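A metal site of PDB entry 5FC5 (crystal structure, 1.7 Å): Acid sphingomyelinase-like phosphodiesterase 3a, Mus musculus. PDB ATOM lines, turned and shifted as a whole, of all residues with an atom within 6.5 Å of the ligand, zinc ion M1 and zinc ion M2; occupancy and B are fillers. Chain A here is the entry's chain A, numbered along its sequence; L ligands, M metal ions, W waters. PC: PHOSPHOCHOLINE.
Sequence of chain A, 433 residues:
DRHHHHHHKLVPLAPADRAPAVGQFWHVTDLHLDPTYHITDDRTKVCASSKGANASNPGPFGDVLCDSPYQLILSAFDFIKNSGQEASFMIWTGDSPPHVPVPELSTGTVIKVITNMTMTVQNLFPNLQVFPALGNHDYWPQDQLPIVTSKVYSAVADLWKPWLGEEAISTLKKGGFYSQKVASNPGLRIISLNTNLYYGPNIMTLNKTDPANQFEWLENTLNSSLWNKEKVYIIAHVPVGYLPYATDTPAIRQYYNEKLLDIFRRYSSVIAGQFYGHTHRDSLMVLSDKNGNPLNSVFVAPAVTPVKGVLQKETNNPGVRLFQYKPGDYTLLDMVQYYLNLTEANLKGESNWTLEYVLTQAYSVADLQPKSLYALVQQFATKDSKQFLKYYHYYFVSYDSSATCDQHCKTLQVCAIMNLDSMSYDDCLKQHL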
ATOM      1  N   ASP A  30      13.170  19.651   0.684  1.00  0.00           N
ATOM      2  CA  ASP A  30      12.332  19.824  -0.504  1.00  0.00           C
ATOM      3  C   ASP A  30      12.929  19.138  -1.737  1.00  0.00           C
ATOM      4  O   ASP A  30      13.163  19.731  -2.783  1.00  0.00           O
ATOM      5  CB  ASP A  30      12.095  21.319  -0.728  1.00  0.00           C
ATOM      6  CG  ASP A  30      11.213  21.920   0.368  1.00  0.00           C
ATOM      7  OD1 ASP A  30      11.729  22.306   1.440  1.00  0.00           O
ATOM      8  OD2 ASP A  30       9.973  21.938   0.202  1.00  0.00           O
ATOM      9  N   LEU A  31      13.154  17.833  -1.585  1.00  0.00           N
ATOM     10  CA  LEU A  31      13.720  17.007  -2.644  1.00  0.00           C
ATOM     11  C   LEU A  31      12.735  16.843  -3.796  1.00  0.00           C
ATOM     12  O   LEU A  31      13.133  16.885  -4.954  1.00  0.00           O
ATOM     13  CB  LEU A  31      14.112  15.642  -2.077  1.00  0.00           C
ATOM     14  CG  LEU A  31      15.118  15.677  -0.933  1.00  0.00           C
ATOM     15  CD1 LEU A  31      15.254  14.270  -0.356  1.00  0.00           C
ATOM     16  CD2 LEU A  31      16.435  16.216  -1.390  1.00  0.00           C
ATOM     17  N   HIS A  32      11.430  16.669  -3.491  1.00  0.00           N
ATOM     18  CA  HIS A  32      10.363  16.551  -4.490  1.00  0.00           C
ATOM     19  C   HIS A  32      10.775  15.672  -5.661  1.00  0.00           C
ATOM     20  O   HIS A  32      10.918  16.158  -6.788  1.00  0.00           O
ATOM     21  CB  HIS A  32       9.970  17.934  -4.980  1.00  0.00           C
ATOM     22  CG  HIS A  32       9.279  18.758  -3.941  1.00  0.00           C
ATOM     23  ND1 HIS A  32       8.012  18.446  -3.501  1.00  0.00           N
ATOM     24  CD2 HIS A  32       9.657  19.868  -3.285  1.00  0.00           C
ATOM     25  CE1 HIS A  32       7.637  19.335  -2.592  1.00  0.00           C
ATOM     26  NE2 HIS A  32       8.610  20.232  -2.473  1.00  0.00           N
ATOM     27  N   GLY A  94      11.827  17.755   4.794  1.00  0.00           N
ATOM     28  CA  GLY A  94      10.560  17.265   4.259  1.00  0.00           C
ATOM     29  C   GLY A  94      10.322  17.577   2.790  1.00  0.00           C
ATOM     30  O   GLY A  94      11.165  18.132   2.093  1.00  0.00           O
ATOM     31  N   ASP A  95       9.098  17.201   2.348  1.00  0.00           N
ATOM     32  CA  ASP A  95       8.527  17.415   1.015  1.00  0.00           C
ATOM     33  C   ASP A  95       9.186  16.558  -0.077  1.00  0.00           C
ATOM     34  O   ASP A  95       9.923  17.096  -0.934  1.00  0.00           O
ATOM     35  CB  ASP A  95       8.596  18.904   0.624  1.00  0.00           C
ATOM     36  CG  ASP A  95       7.268  19.602   0.817  1.00  0.00           C
ATOM     37  OD1 ASP A  95       6.353  19.023   1.442  1.00  0.00           O
ATOM     38  OD2 ASP A  95       7.132  20.757   0.349  1.00  0.00           O
ATOM     39  N   HIS A  99       5.010  17.638  -7.220  1.00  0.00           N
ATOM     40  CA  HIS A  99       3.824  18.506  -7.337  1.00  0.00           C
ATOM     41  C   HIS A  99       2.977  18.008  -8.516  1.00  0.00           C
ATOM     42  O   HIS A  99       3.195  18.385  -9.671  1.00  0.00           O
ATOM     43  CB  HIS A  99       4.170  19.978  -7.521  1.00  0.00           C
ATOM     44  CG  HIS A  99       4.989  20.556  -6.416  1.00  0.00           C
ATOM     45  ND1 HIS A  99       6.339  20.307  -6.282  1.00  0.00           N
ATOM     46  CD2 HIS A  99       4.652  21.409  -5.411  1.00  0.00           C
ATOM     47  CE1 HIS A  99       6.802  20.958  -5.225  1.00  0.00           C
ATOM     48  NE2 HIS A  99       5.798  21.628  -4.671  1.00  0.00           N
ATOM     49  N   GLY A 135       7.008  17.234   5.563  1.00  0.00           N
ATOM     50  CA  GLY A 135       6.510  18.371   4.798  1.00  0.00           C
ATOM     51  C   GLY A 135       5.049  18.197   4.422  1.00  0.00           C
ATOM     52  O   GLY A 135       4.444  17.128   4.583  1.00  0.00           O
ATOM     53  N   ASN A 136       4.469  19.274   3.881  1.00  0.00           N
ATOM     54  CA  ASN A 136       3.035  19.240   3.600  1.00  0.00           C
ATOM     55  C   ASN A 136       2.726  18.297   2.450  1.00  0.00           C
ATOM     56  O   ASN A 136       1.606  17.778   2.389  1.00  0.00           O
ATOM     57  CB  ASN A 136       2.532  20.658   3.346  1.00  0.00           C
ATOM     58  CG  ASN A 136       3.316  21.378   2.269  1.00  0.00           C
ATOM     59  OD1 ASN A 136       4.520  21.653   2.424  1.00  0.00           O
ATOM     60  ND2 ASN A 136       2.667  21.674   1.174  1.00  0.00           N
ATOM     61  N   HIS A 137       3.693  18.003   1.589  1.00  0.00           N
ATOM     62  CA  HIS A 137       3.445  17.027   0.560  1.00  0.00           C
ATOM     63  C   HIS A 137       3.681  15.597   1.019  1.00  0.00           C
ATOM     64  O   HIS A 137       3.380  14.670   0.258  1.00  0.00           O
ATOM     65  CB  HIS A 137       4.323  17.340  -0.649  1.00  0.00           C
ATOM     66  CG  HIS A 137       3.874  18.549  -1.398  1.00  0.00           C
ATOM     67  ND1 HIS A 137       2.949  18.476  -2.423  1.00  0.00           N
ATOM     68  CD2 HIS A 137       4.163  19.859  -1.241  1.00  0.00           C
ATOM     69  CE1 HIS A 137       2.714  19.691  -2.889  1.00  0.00           C
ATOM     70  NE2 HIS A 137       3.449  20.555  -2.205  1.00  0.00           N
ATOM     71  N   GLN A 142      -2.293  15.836  -0.198  1.00  0.00           N
ATOM     72  CA  GLN A 142      -1.304  16.797   0.258  1.00  0.00           C
ATOM     73  C   GLN A 142      -1.950  17.798   1.198  1.00  0.00           C
ATOM     74  O   GLN A 142      -3.141  18.149   1.078  1.00  0.00           O
ATOM     75  CB  GLN A 142      -0.667  17.528  -0.922  1.00  0.00           C
ATOM     76  CG  GLN A 142      -1.576  18.484  -1.687  1.00  0.00           C
ATOM     77  CD  GLN A 142      -0.818  19.371  -2.648  1.00  0.00           C
ATOM     78  OE1 GLN A 142      -0.433  18.934  -3.744  1.00  0.00           O
ATOM     79  NE2 GLN A 142      -0.558  20.614  -2.234  1.00  0.00           N
ATOM     80  N   ASP A 143      -1.128  18.248   2.149  1.00  0.00           N
ATOM     81  CA  ASP A 143      -1.437  19.273   3.141  1.00  0.00           C
ATOM     82  C   ASP A 143      -2.419  18.814   4.216  1.00  0.00           C
ATOM     83  O   ASP A 143      -2.622  19.539   5.197  1.00  0.00           O
ATOM     84  CB  ASP A 143      -2.012  20.533   2.490  1.00  0.00           C
ATOM     85  CG  ASP A 143      -1.205  21.023   1.310  1.00  0.00           C
ATOM     86  OD1 ASP A 143       0.041  20.898   1.300  1.00  0.00           O
ATOM     87  OD2 ASP A 143      -1.843  21.554   0.357  1.00  0.00           O
ATOM     88  N   ASN A 196       3.142  21.564   9.501  1.00  0.00           N
ATOM     89  CA  ASN A 196       2.048  21.401   8.556  1.00  0.00           C
ATOM     90  C   ASN A 196       0.693  21.349   9.256  1.00  0.00           C
ATOM     91  O   ASN A 196      -0.338  21.525   8.586  1.00  0.00           O
ATOM     92  CB  ASN A 196       2.281  20.137   7.731  1.00  0.00           C
ATOM     93  CG  ASN A 196       3.677  20.047   7.220  1.00  0.00           C
ATOM     94  OD1 ASN A 196       4.081  20.803   6.332  1.00  0.00           O
ATOM     95  ND2 ASN A 196       4.437  19.166   7.780  1.00  0.00           N
ATOM     96  N   TYR A 199      -0.464  24.885   8.722  1.00  0.00           N
ATOM     97  CA  TYR A 199      -0.456  25.393   7.353  1.00  0.00           C
ATOM     98  C   TYR A 199      -1.895  25.584   6.838  1.00  0.00           C
ATOM     99  O   TYR A 199      -2.765  24.737   7.018  1.00  0.00           O
ATOM    100  CB  TYR A 199       0.362  24.407   6.474  1.00  0.00           C
ATOM    101  CG  TYR A 199       0.653  24.809   5.077  1.00  0.00           C
ATOM    102  CD1 TYR A 199       1.087  26.081   4.742  1.00  0.00           C
ATOM    103  CD2 TYR A 199       0.497  23.877   4.052  1.00  0.00           C
ATOM    104  CE1 TYR A 199       1.365  26.399   3.448  1.00  0.00           C
ATOM    105  CE2 TYR A 199       0.766  24.201   2.750  1.00  0.00           C
ATOM    106  CZ  TYR A 199       1.198  25.455   2.450  1.00  0.00           C
ATOM    107  OH  TYR A 199       1.445  25.775   1.145  1.00  0.00           O
ATOM    108  N   HIS A 237       9.164  21.947   8.590  1.00  0.00           N
ATOM    109  CA  HIS A 237       9.004  22.186   7.156  1.00  0.00           C
ATOM    110  C   HIS A 237       8.558  23.628   6.916  1.00  0.00           C
ATOM    111  O   HIS A 237       9.351  24.442   6.436  1.00  0.00           O
ATOM    112  CB  HIS A 237       8.052  21.165   6.527  1.00  0.00           C
ATOM    113  CG  HIS A 237       7.917  21.343   5.063  1.00  0.00           C
ATOM    114  ND1 HIS A 237       8.961  21.127   4.168  1.00  0.00           N
ATOM    115  CD2 HIS A 237       6.884  21.800   4.321  1.00  0.00           C
ATOM    116  CE1 HIS A 237       8.563  21.430   2.955  1.00  0.00           C
ATOM    117  NE2 HIS A 237       7.297  21.816   3.006  1.00  0.00           N
ATOM    118  N   VAL A 238       7.307  23.960   7.221  1.00  0.00           N
ATOM    119  CA  VAL A 238       6.791  25.317   7.002  1.00  0.00           C
ATOM    120  C   VAL A 238       7.366  26.217   8.100  1.00  0.00           C
ATOM    121  O   VAL A 238       7.324  25.841   9.276  1.00  0.00           O
ATOM    122  CB  VAL A 238       5.266  25.336   7.023  1.00  0.00           C
ATOM    123  CG1 VAL A 238       4.739  26.732   6.644  1.00  0.00           C
ATOM    124  CG2 VAL A 238       4.744  24.253   6.116  1.00  0.00           C
ATOM    125  N   LEU A 243       5.652  35.574   4.715  1.00  0.00           N
ATOM    126  CA  LEU A 243       6.163  35.352   3.363  1.00  0.00           C
ATOM    127  C   LEU A 243       6.950  36.585   2.903  1.00  0.00           C
ATOM    128  O   LEU A 243       6.476  37.703   3.059  1.00  0.00           O
ATOM    129  CB  LEU A 243       5.036  35.106   2.375  1.00  0.00           C
ATOM    130  CG  LEU A 243       4.079  33.953   2.632  1.00  0.00           C
ATOM    131  CD1 LEU A 243       3.044  33.878   1.489  1.00  0.00           C
ATOM    132  CD2 LEU A 243       4.838  32.701   2.748  1.00  0.00           C
ATOM    133  N   TYR A 245       7.739  37.580  -0.053  1.00  0.00           N
ATOM    134  CA  TYR A 245       7.385  37.987  -1.423  1.00  0.00           C
ATOM    135  C   TYR A 245       5.946  38.421  -1.536  1.00  0.00           C
ATOM    136  O   TYR A 245       5.472  38.682  -2.651  1.00  0.00           O
ATOM    137  CB  TYR A 245       7.619  36.809  -2.395  1.00  0.00           C
ATOM    138  CG  TYR A 245       6.861  35.551  -2.035  1.00  0.00           C
ATOM    139  CD1 TYR A 245       7.462  34.583  -1.225  1.00  0.00           C
ATOM    140  CD2 TYR A 245       5.578  35.327  -2.494  1.00  0.00           C
ATOM    141  CE1 TYR A 245       6.781  33.436  -0.850  1.00  0.00           C
ATOM    142  CE2 TYR A 245       4.893  34.171  -2.146  1.00  0.00           C
ATOM    143  CZ  TYR A 245       5.513  33.235  -1.318  1.00  0.00           C
ATOM    144  OH  TYR A 245       4.871  32.130  -0.977  1.00  0.00           O
ATOM    145  N   GLY A 277      12.308  24.651   5.807  1.00  0.00           N
ATOM    146  CA  GLY A 277      12.285  24.500   4.363  1.00  0.00           C
ATOM    147  C   GLY A 277      11.016  25.130   3.808  1.00  0.00           C
ATOM    148  O   GLY A 277      10.681  26.257   4.190  1.00  0.00           O
ATOM    149  N   HIS A 278      10.351  24.411   2.898  1.00  0.00           N
ATOM    150  CA  HIS A 278       9.080  24.784   2.259  1.00  0.00           C
ATOM    151  C   HIS A 278       9.085  25.940   1.248  1.00  0.00           C
ATOM    152  O   HIS A 278       8.390  25.879   0.241  1.00  0.00           O
ATOM    153  CB  HIS A 278       8.051  25.102   3.352  1.00  0.00           C
ATOM    154  CG  HIS A 278       6.690  25.414   2.811  1.00  0.00           C
ATOM    155  ND1 HIS A 278       5.881  24.475   2.197  1.00  0.00           N
ATOM    156  CD2 HIS A 278       5.989  26.565   2.838  1.00  0.00           C
ATOM    157  CE1 HIS A 278       4.748  25.056   1.848  1.00  0.00           C
ATOM    158  NE2 HIS A 278       4.783  26.318   2.227  1.00  0.00           N
ATOM    159  N   THR A 279       9.810  27.017   1.502  1.00  0.00           N
ATOM    160  CA  THR A 279       9.738  28.158   0.626  1.00  0.00           C
ATOM    161  C   THR A 279      10.534  27.953  -0.657  1.00  0.00           C
ATOM    162  O   THR A 279      10.243  28.620  -1.647  1.00  0.00           O
ATOM    163  CB  THR A 279      10.263  29.404   1.324  1.00  0.00           C
ATOM    164  OG1 THR A 279      11.677  29.319   1.399  1.00  0.00           O
ATOM    165  CG2 THR A 279       9.645  29.546   2.730  1.00  0.00           C
ATOM    166  N   HIS A 280      11.467  27.005  -0.682  1.00  0.00           N
ATOM    167  CA  HIS A 280      12.353  26.747  -1.819  1.00  0.00           C
ATOM    168  C   HIS A 280      13.281  27.916  -2.092  1.00  0.00           C
ATOM    169  O   HIS A 280      13.855  28.037  -3.201  1.00  0.00           O
ATOM    170  CB  HIS A 280      11.551  26.376  -3.067  1.00  0.00           C
ATOM    171  CG  HIS A 280      10.773  25.104  -2.961  1.00  0.00           C
ATOM    172  ND1 HIS A 280      10.342  24.432  -4.083  1.00  0.00           N
ATOM    173  CD2 HIS A 280      10.337  24.383  -1.901  1.00  0.00           C
ATOM    174  CE1 HIS A 280       9.648  23.366  -3.724  1.00  0.00           C
ATOM    175  NE2 HIS A 280       9.637  23.304  -2.389  1.00  0.00           N
ATOM    176  N   ALA A 303      15.500  24.655  -1.847  1.00  0.00           N
ATOM    177  CA  ALA A 303      15.176  23.285  -2.183  1.00  0.00           C
ATOM    178  C   ALA A 303      16.238  22.656  -3.094  1.00  0.00           C
ATOM    179  O   ALA A 303      16.966  23.343  -3.809  1.00  0.00           O
ATOM    180  CB  ALA A 303      13.846  23.245  -2.909  1.00  0.00           C
ATOM    181  N   THR A 305      14.795  20.620  -5.513  1.00  0.00           N
ATOM    182  CA  THR A 305      14.022  20.774  -6.741  1.00  0.00           C
ATOM    183  C   THR A 305      14.153  22.203  -7.248  1.00  0.00           C
ATOM    184  O   THR A 305      14.205  23.150  -6.445  1.00  0.00           O
ATOM    185  CB  THR A 305      12.555  20.421  -6.567  1.00  0.00           C
ATOM    186  OG1 THR A 305      11.898  20.558  -7.843  1.00  0.00           O
ATOM    187  CG2 THR A 305      11.823  21.387  -5.559  1.00  0.00           C
ATOM    188  N   VAL A 307      11.765  23.406  -9.354  1.00  0.00           N
ATOM    189  CA  VAL A 307      10.465  23.561  -9.981  1.00  0.00           C
ATOM    190  C   VAL A 307       9.871  24.945  -9.764  1.00  0.00           C
ATOM    191  O   VAL A 307      10.007  25.551  -8.680  1.00  0.00           O
ATOM    192  CB  VAL A 307       9.507  22.468  -9.481  1.00  0.00           C
ATOM    193  CG1 VAL A 307       9.068  22.738  -7.990  1.00  0.00           C
ATOM    194  CG2 VAL A 307       8.299  22.336 -10.382  1.00  0.00           C
ATOM    195  N   GLN A 312       5.450  32.004 -12.874  1.00  0.00           N
ATOM    196  CA  GLN A 312       6.549  32.605 -12.135  1.00  0.00           C
ATOM    197  C   GLN A 312       7.677  32.985 -13.063  1.00  0.00           C
ATOM    198  O   GLN A 312       8.006  32.259 -13.994  1.00  0.00           O
ATOM    199  CB  GLN A 312       7.092  31.628 -11.075  1.00  0.00           C
ATOM    200  CG  GLN A 312       6.156  31.273  -9.979  1.00  0.00           C
ATOM    201  CD  GLN A 312       6.784  30.175  -9.087  1.00  0.00           C
ATOM    202  OE1 GLN A 312       6.258  29.070  -9.008  1.00  0.00           O
ATOM    203  NE2 GLN A 312       7.967  30.468  -8.509  1.00  0.00           N
HETATM  204  P1   PC L   1       5.460  23.301  -1.472  1.00  0.00           P
HETATM  205  O1   PC L   1       4.282  23.140  -2.443  1.00  0.00           O
HETATM  206  O3   PC L   1       6.605  22.617  -2.026  1.00  0.00           O
HETATM  207  O4   PC L   1       4.920  22.695  -0.203  1.00  0.00           O
HETATM  208  O2   PC L   1       5.664  24.897  -1.265  1.00  0.00           O
HETATM  209  C1   PC L   1       6.492  25.538  -2.189  1.00  0.00           C
HETATM  210  C2   PC L   1       6.360  27.078  -2.039  1.00  0.00           C
HETATM  211  N1   PC L   1       5.118  27.600  -2.601  1.00  0.00           N
HETATM  212  C3   PC L   1       3.914  27.165  -1.862  1.00  0.00           C
HETATM  213  C4   PC L   1       5.000  27.256  -4.024  1.00  0.00           C
HETATM  214  C5   PC L   1       5.208  29.052  -2.528  1.00  0.00           C
HETATM  215 ZN    ZN M   1       6.121  22.484   1.501  1.00  0.00          ZN
HETATM  216 ZN    ZN M   2       8.520  21.922  -1.247  1.00  0.00          ZN
HETATM  217  O   HOH W   1       7.560  23.522  -0.122  1.00  0.00           O
HETATM  218  O   HOH W   2       6.448  30.085   0.463  1.00  0.00           O
HETATM  219  O   HOH W   3       3.182  28.465   1.162  1.00  0.00           O
HETATM  220  O   HOH W   4       3.068  24.716  -5.219  1.00  0.00           O
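NE2 of His 137 lies within hydrogen-bond range of O1 of the ligand (2.7 Å). NE2 of His 99 is in hydrogen-bond range of O1 of the ligand.
N of Gly 277 sits at hydrogen-bond distance from O of His 237 (3.0 Å). The side-chain amide nitrogen (ND2) of Asn 136 lies within hydrogen-bond range of the side-chain carboxylate (OD1) of Asp 143 (2.7 Å). N of Asn 136 lies within hydrogen-bond range of OD1 of Asn 196, at 2.9 Å. OD1 of Asp 30 sits at hydrogen-bond distance from N of His 278 (2.9 Å). The backbone NH (N) of Thr 305 sits at hydrogen-bond distance from the backbone carbonyl oxygen (O) of Asp 30 (3.3 Å). N of Asp 30 lies within hydrogen-bond range of O of Gly 94, at 2.9 Å. The side-chain carboxylate (OD1) of Asp 95 sits at hydrogen-bond distance from the backbone NH (N) of His 137 (2.9 Å). O of Asp 95 is in hydrogen-bond range of N of Leu 31 (3.4 Å).
Tyr 245 touches the ligand. Hydrophobic or aromatic side chains that line the ligand: His 32, His 99, His 137, His 278 and His 280. Of the 25 residues printed, 8 come within 4 Å of the ligand.
Of the 25 residues printed, 4 come within 4 Å of zinc ion M2. The nearest printed residue that does not touch zinc ion M2 is His 278 (4.2 Å).
Zinc ion M1 is bound by NE2 of His 237 (2.0 Å), OD1 of Asn 136 (2.0 Å), O4 of the ligand (2.1 Å), ND1 of His 278 (2.1 Å), OD2 of Asp 95 (2.3 Å) and water W1 (2.4 Å). Zinc ion M1 has six donor atoms within binding distance.
Zinc ion M2 is bound by the side-chain carboxylate (OD2) of Asp 30 (2.1 Å), a ring nitrogen (NE2) of His 32 (2.1 Å), a ring nitrogen (NE2) of His 280 (2.1 Å), water W1 (2.2 Å), an oxygen (O3) of the ligand (2.2 Å) and the side-chain carboxylate (OD2) of Asp 95 (2.4 Å).
Water W1 bridges the backbone carbonyl oxygen of His 278 (2.5 Å) and an oxygen (O2) of the ligand (2.6 Å). Water W3 bridges NE2 of His 278 (2.9 Å) and OH of Tyr 199 (3.2 Å).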
